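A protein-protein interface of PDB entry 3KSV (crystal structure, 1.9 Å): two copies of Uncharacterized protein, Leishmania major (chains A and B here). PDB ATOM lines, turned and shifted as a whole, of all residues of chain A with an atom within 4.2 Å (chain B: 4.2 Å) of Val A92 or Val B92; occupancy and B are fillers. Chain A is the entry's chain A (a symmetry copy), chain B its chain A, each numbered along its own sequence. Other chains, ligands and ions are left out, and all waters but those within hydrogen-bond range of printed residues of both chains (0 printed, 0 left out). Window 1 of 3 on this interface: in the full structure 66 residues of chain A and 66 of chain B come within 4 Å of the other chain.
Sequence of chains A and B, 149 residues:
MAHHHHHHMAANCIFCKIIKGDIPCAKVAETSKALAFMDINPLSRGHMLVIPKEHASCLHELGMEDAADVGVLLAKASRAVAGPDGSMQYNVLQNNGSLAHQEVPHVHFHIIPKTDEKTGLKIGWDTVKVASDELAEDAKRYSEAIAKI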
ATOM      1  N   LEU A  59     -20.534 -32.685  16.400  1.00  0.00           N
ATOM      2  CA  LEU A  59     -21.944 -32.829  16.726  1.00  0.00           C
ATOM      3  C   LEU A  59     -22.295 -34.263  17.072  1.00  0.00           C
ATOM      4  O   LEU A  59     -23.164 -34.504  17.923  1.00  0.00           O
ATOM      5  CB  LEU A  59     -22.828 -32.324  15.570  1.00  0.00           C
ATOM      6  CG  LEU A  59     -24.321 -32.200  15.879  1.00  0.00           C
ATOM      7  CD1 LEU A  59     -24.566 -31.253  17.044  1.00  0.00           C
ATOM      8  CD2 LEU A  59     -25.117 -31.739  14.628  1.00  0.00           C
ATOM      9  N   LEU A  74     -31.350 -23.090  19.770  1.00  0.00           N
ATOM     10  CA  LEU A  74     -31.093 -22.632  18.391  1.00  0.00           C
ATOM     11  C   LEU A  74     -32.337 -21.981  17.749  1.00  0.00           C
ATOM     12  O   LEU A  74     -32.259 -20.910  17.129  1.00  0.00           O
ATOM     13  CB  LEU A  74     -30.627 -23.808  17.546  1.00  0.00           C
ATOM     14  CG  LEU A  74     -30.069 -23.527  16.155  1.00  0.00           C
ATOM     15  CD1 LEU A  74     -28.847 -22.614  16.234  1.00  0.00           C
ATOM     16  CD2 LEU A  74     -29.717 -24.868  15.485  1.00  0.00           C
ATOM     17  N   ASN A  91     -28.259 -17.428   8.082  1.00  0.00           N
ATOM     18  CA  ASN A  91     -27.776 -18.776   7.874  1.00  0.00           C
ATOM     19  C   ASN A  91     -27.384 -19.383   9.225  1.00  0.00           C
ATOM     20  O   ASN A  91     -26.842 -18.681  10.106  1.00  0.00           O
ATOM     21  CB  ASN A  91     -26.580 -18.786   6.935  1.00  0.00           C
ATOM     22  CG  ASN A  91     -26.927 -18.340   5.525  1.00  0.00           C
ATOM     23  OD1 ASN A  91     -26.742 -17.173   5.189  1.00  0.00           O
ATOM     24  ND2 ASN A  91     -27.417 -19.263   4.686  1.00  0.00           N
ATOM     25  N   VAL A  92     -27.699 -20.671   9.391  1.00  0.00           N
ATOM     26  CA  VAL A  92     -27.246 -21.452  10.523  1.00  0.00           C
ATOM     27  C   VAL A  92     -26.166 -22.415  10.000  1.00  0.00           C
ATOM     28  O   VAL A  92     -26.381 -23.160   9.050  1.00  0.00           O
ATOM     29  CB  VAL A  92     -28.398 -22.234  11.189  1.00  0.00           C
ATOM     30  CG1 VAL A  92     -27.853 -23.129  12.323  1.00  0.00           C
ATOM     31  CG2 VAL A  92     -29.444 -21.254  11.747  1.00  0.00           C
ATOM     32  N   LEU A  93     -24.999 -22.378  10.638  1.00  0.00           N
ATOM     33  CA  LEU A  93     -23.840 -23.109  10.198  1.00  0.00           C
ATOM     34  C   LEU A  93     -23.149 -23.736  11.388  1.00  0.00           C
ATOM     35  O   LEU A  93     -22.885 -23.074  12.380  1.00  0.00           O
ATOM     36  CB  LEU A  93     -22.863 -22.176   9.504  1.00  0.00           C
ATOM     37  CG  LEU A  93     -21.587 -22.850   8.989  1.00  0.00           C
ATOM     38  CD1 LEU A  93     -21.939 -23.737   7.786  1.00  0.00           C
ATOM     39  CD2 LEU A  93     -20.578 -21.790   8.627  1.00  0.00           C
ATOM     40  N   GLN A  94     -22.832 -25.029  11.282  1.00  0.00           N
ATOM     41  CA  GLN A  94     -22.086 -25.720  12.339  1.00  0.00           C
ATOM     42  C   GLN A  94     -21.081 -26.623  11.670  1.00  0.00           C
ATOM     43  O   GLN A  94     -21.453 -27.473  10.878  1.00  0.00           O
ATOM     44  CB  GLN A  94     -23.034 -26.514  13.217  1.00  0.00           C
ATOM     45  CG  GLN A  94     -22.407 -27.033  14.508  1.00  0.00           C
ATOM     46  CD  GLN A  94     -21.868 -28.422  14.357  1.00  0.00           C
ATOM     47  OE1 GLN A  94     -22.482 -29.250  13.685  1.00  0.00           O
ATOM     48  NE2 GLN A  94     -20.693 -28.696  14.967  1.00  0.00           N
ATOM     49  N   ASN A  96     -17.660 -29.277  11.511  1.00  0.00           N
ATOM     50  CA  ASN A  96     -17.189 -30.468  12.197  1.00  0.00           C
ATOM     51  C   ASN A  96     -15.936 -30.979  11.528  1.00  0.00           C
ATOM     52  O   ASN A  96     -16.013 -31.667  10.530  1.00  0.00           O
ATOM     53  CB  ASN A  96     -18.264 -31.523  12.188  1.00  0.00           C
ATOM     54  CG  ASN A  96     -19.504 -31.069  12.906  1.00  0.00           C
ATOM     55  OD1 ASN A  96     -19.600 -31.189  14.117  1.00  0.00           O
ATOM     56  ND2 ASN A  96     -20.468 -30.541  12.151  1.00  0.00           N
ATOM     57  N   PHE A 109     -22.881 -23.568  16.928  1.00  0.00           N
ATOM     58  CA  PHE A 109     -23.767 -23.177  15.850  1.00  0.00           C
ATOM     59  C   PHE A 109     -23.676 -21.670  15.657  1.00  0.00           C
ATOM     60  O   PHE A 109     -23.956 -20.911  16.564  1.00  0.00           O
ATOM     61  CB  PHE A 109     -25.217 -23.553  16.188  1.00  0.00           C
ATOM     62  CG  PHE A 109     -25.509 -25.001  16.058  1.00  0.00           C
ATOM     63  CD1 PHE A 109     -26.092 -25.495  14.895  1.00  0.00           C
ATOM     64  CD2 PHE A 109     -25.181 -25.879  17.078  1.00  0.00           C
ATOM     65  CE1 PHE A 109     -26.348 -26.808  14.755  1.00  0.00           C
ATOM     66  CE2 PHE A 109     -25.440 -27.222  16.946  1.00  0.00           C
ATOM     67  CZ  PHE A 109     -26.040 -27.694  15.782  1.00  0.00           C
ATOM     68  N   HIS A 110     -23.278 -21.245  14.472  1.00  0.00           N
ATOM     69  CA  HIS A 110     -23.324 -19.848  14.093  1.00  0.00           C
ATOM     70  C   HIS A 110     -24.760 -19.553  13.625  1.00  0.00           C
ATOM     71  O   HIS A 110     -25.334 -20.360  12.860  1.00  0.00           O
ATOM     72  CB  HIS A 110     -22.378 -19.598  12.914  1.00  0.00           C
ATOM     73  CG  HIS A 110     -20.933 -19.931  13.173  1.00  0.00           C
ATOM     74  ND1 HIS A 110     -20.014 -18.985  13.560  1.00  0.00           N
ATOM     75  CD2 HIS A 110     -20.236 -21.086  13.009  1.00  0.00           C
ATOM     76  CE1 HIS A 110     -18.823 -19.549  13.657  1.00  0.00           C
ATOM     77  NE2 HIS A 110     -18.930 -20.825  13.331  1.00  0.00           N
ATOM     78  N   LEU B  59     -36.530 -21.155  10.456  1.00  0.00           N
ATOM     79  CA  LEU B  59     -36.307 -21.837  11.720  1.00  0.00           C
ATOM     80  C   LEU B  59     -37.061 -21.172  12.855  1.00  0.00           C
ATOM     81  O   LEU B  59     -37.519 -21.856  13.784  1.00  0.00           O
ATOM     82  CB  LEU B  59     -34.803 -21.911  12.044  1.00  0.00           C
ATOM     83  CG  LEU B  59     -34.419 -22.807  13.223  1.00  0.00           C
ATOM     84  CD1 LEU B  59     -34.874 -24.241  12.996  1.00  0.00           C
ATOM     85  CD2 LEU B  59     -32.891 -22.758  13.492  1.00  0.00           C
ATOM     86  N   LEU B  74     -30.988 -34.422  14.156  1.00  0.00           N
ATOM     87  CA  LEU B  74     -29.767 -33.851  13.554  1.00  0.00           C
ATOM     88  C   LEU B  74     -28.481 -34.472  14.138  1.00  0.00           C
ATOM     89  O   LEU B  74     -27.551 -34.842  13.407  1.00  0.00           O
ATOM     90  CB  LEU B  74     -29.758 -32.344  13.762  1.00  0.00           C
ATOM     91  CG  LEU B  74     -28.721 -31.514  13.013  1.00  0.00           C
ATOM     92  CD1 LEU B  74     -28.876 -31.684  11.503  1.00  0.00           C
ATOM     93  CD2 LEU B  74     -28.879 -30.039  13.425  1.00  0.00           C
ATOM     94  N   ASN B  91     -20.245 -30.453   7.297  1.00  0.00           N
ATOM     95  CA  ASN B  91     -20.835 -29.179   7.649  1.00  0.00           C
ATOM     96  C   ASN B  91     -22.350 -29.354   7.803  1.00  0.00           C
ATOM     97  O   ASN B  91     -22.984 -30.119   7.044  1.00  0.00           O
ATOM     98  CB  ASN B  91     -20.539 -28.131   6.588  1.00  0.00           C
ATOM     99  CG  ASN B  91     -19.063 -27.791   6.483  1.00  0.00           C
ATOM    100  OD1 ASN B  91     -18.366 -28.343   5.637  1.00  0.00           O
ATOM    101  ND2 ASN B  91     -18.578 -26.871   7.329  1.00  0.00           N
ATOM    102  N   VAL B  92     -22.909 -28.675   8.808  1.00  0.00           N
ATOM    103  CA  VAL B  92     -24.342 -28.576   8.990  1.00  0.00           C
ATOM    104  C   VAL B  92     -24.745 -27.142   8.606  1.00  0.00           C
ATOM    105  O   VAL B  92     -24.201 -26.167   9.114  1.00  0.00           O
ATOM    106  CB  VAL B  92     -24.768 -28.892  10.440  1.00  0.00           C
ATOM    107  CG1 VAL B  92     -26.287 -28.676  10.611  1.00  0.00           C
ATOM    108  CG2 VAL B  92     -24.400 -30.344  10.790  1.00  0.00           C
ATOM    109  N   LEU B  93     -25.706 -27.036   7.692  1.00  0.00           N
ATOM    110  CA  LEU B  93     -26.110 -25.778   7.119  1.00  0.00           C
ATOM    111  C   LEU B  93     -27.618 -25.721   7.024  1.00  0.00           C
ATOM    112  O   LEU B  93     -28.251 -26.639   6.527  1.00  0.00           O
ATOM    113  CB  LEU B  93     -25.528 -25.626   5.724  1.00  0.00           C
ATOM    114  CG  LEU B  93     -25.892 -24.318   5.016  1.00  0.00           C
ATOM    115  CD1 LEU B  93     -25.149 -23.158   5.693  1.00  0.00           C
ATOM    116  CD2 LEU B  93     -25.541 -24.430   3.555  1.00  0.00           C
ATOM    117  N   GLN B  94     -28.203 -24.614   7.491  1.00  0.00           N
ATOM    118  CA  GLN B  94     -29.652 -24.412   7.375  1.00  0.00           C
ATOM    119  C   GLN B  94     -29.881 -22.969   7.003  1.00  0.00           C
ATOM    120  O   GLN B  94     -29.448 -22.077   7.716  1.00  0.00           O
ATOM    121  CB  GLN B  94     -30.335 -24.754   8.685  1.00  0.00           C
ATOM    122  CG  GLN B  94     -31.855 -24.857   8.591  1.00  0.00           C
ATOM    123  CD  GLN B  94     -32.531 -23.563   8.926  1.00  0.00           C
ATOM    124  OE1 GLN B  94     -32.094 -22.858   9.834  1.00  0.00           O
ATOM    125  NE2 GLN B  94     -33.605 -23.219   8.180  1.00  0.00           N
ATOM    126  N   ASN B  96     -32.212 -19.557   5.703  1.00  0.00           N
ATOM    127  CA  ASN B  96     -33.463 -18.908   6.062  1.00  0.00           C
ATOM    128  C   ASN B  96     -33.622 -17.636   5.264  1.00  0.00           C
ATOM    129  O   ASN B  96     -33.068 -16.616   5.623  1.00  0.00           O
ATOM    130  CB  ASN B  96     -33.483 -18.616   7.539  1.00  0.00           C
ATOM    131  CG  ASN B  96     -33.392 -19.870   8.362  1.00  0.00           C
ATOM    132  OD1 ASN B  96     -34.395 -20.515   8.624  1.00  0.00           O
ATOM    133  ND2 ASN B  96     -32.175 -20.221   8.777  1.00  0.00           N
ATOM    134  N   PHE B 109     -32.177 -28.875   7.238  1.00  0.00           N
ATOM    135  CA  PHE B 109     -30.784 -28.914   7.637  1.00  0.00           C
ATOM    136  C   PHE B 109     -30.023 -29.828   6.687  1.00  0.00           C
ATOM    137  O   PHE B 109     -30.332 -30.997   6.570  1.00  0.00           O
ATOM    138  CB  PHE B 109     -30.654 -29.456   9.067  1.00  0.00           C
ATOM    139  CG  PHE B 109     -31.048 -28.486  10.116  1.00  0.00           C
ATOM    140  CD1 PHE B 109     -30.080 -27.724  10.764  1.00  0.00           C
ATOM    141  CD2 PHE B 109     -32.382 -28.308  10.446  1.00  0.00           C
ATOM    142  CE1 PHE B 109     -30.422 -26.827  11.707  1.00  0.00           C
ATOM    143  CE2 PHE B 109     -32.743 -27.396  11.408  1.00  0.00           C
ATOM    144  CZ  PHE B 109     -31.757 -26.656  12.056  1.00  0.00           C
ATOM    145  N   HIS B 110     -29.030 -29.285   6.007  1.00  0.00           N
ATOM    146  CA  HIS B 110     -28.110 -30.073   5.213  1.00  0.00           C
ATOM    147  C   HIS B 110     -27.042 -30.623   6.175  1.00  0.00           C
ATOM    148  O   HIS B 110     -26.535 -29.864   7.030  1.00  0.00           O
ATOM    149  CB  HIS B 110     -27.410 -29.177   4.186  1.00  0.00           C
ATOM    150  CG  HIS B 110     -28.328 -28.476   3.220  1.00  0.00           C
ATOM    151  ND1 HIS B 110     -28.602 -28.974   1.968  1.00  0.00           N
ATOM    152  CD2 HIS B 110     -28.956 -27.274   3.291  1.00  0.00           C
ATOM    153  CE1 HIS B 110     -29.385 -28.126   1.325  1.00  0.00           C
ATOM    154  NE2 HIS B 110     -29.618 -27.086   2.107  1.00  0.00           N
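Among the printed residues, pairs that only touch across the chains: Leu A59 with Leu B74, Leu A74 with Leu B59, Asn A91 with Gln B94, Val A92 with Val B92, Val A92 with Leu B93, Leu A93 with Val B92, Leu A93 with Leu B93 and Gln A94 with Asn B91.
Printed residues of chain B that touch a printed residue of chain A: Leu B59, Leu B74, Asn B91, Val B92, Leu B93 and Gln B94.
ND2 of Asn B96 lies within hydrogen-bond range of OE1 of Gln B94. N of His A110 is in hydrogen-bond range of O of Leu A93, 2.8 Å away. The side-chain amide oxygen (OD1) of Asn B96 is in hydrogen-bond range of the backbone NH (N) of Leu B59, 2.9 Å away. The side-chain amide oxygen (OE1) of Gln A94 sits at hydrogen-bond distance from the side-chain amide nitrogen (ND2) of Asn A96, 2.8 Å away. N of Leu A59 lies within hydrogen-bond range of OD1 of Asn A96 (2.9 Å). O of Leu B93 lies within hydrogen-bond range of N of His B110 (2.8 Å).
Leu A59 touches Leu B74, and with the chains exchanged Leu A74 touches Leu B59. Asn A91 touches Gln B94, and with the chains exchanged Gln A94 touches Asn B91. Val B92 touches its own counterpart, Val A92. Val A92 touches Gln B94, and with the chains exchanged Gln A94 touches Val B92. Of the 10 pairs that touch across the chains among the printed residues, 10 have their exchanged pair printed and touching as well.
Of the printed residues of chain B, Leu A59 touches Leu B74 (3.96 Å). Of chain B, only Val B92 (3.7 Å), Leu B93 (3.3 Å) and Gln B94 (2.8 Å) come within 4 Å of Val A92. Printed residues of chain B within 4 Å of Leu A93: Val B92 and Leu B93. Asn A96 touches none of the printed residues of chain B. Val B92 touches just these residues of chain A: Val A92 (3.7 Å), Leu A93 (3.3 Å) and Gln A94 (2.8 Å). Phe B109 touches none of the printed residues of chain A. The nearest printed residue of chain A that does not touch Val B92 is Leu A59 (4.1 Å). The nearest printed residue of chain A that does not touch Gln B94 is Leu A93 (5.0 Å).
N of Val A92 sits at hydrogen-bond distance from O of Gln B94 (2.8 Å). N of Val B92 sits at hydrogen-bond distance from O of Gln A94, 2.8 Å away.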
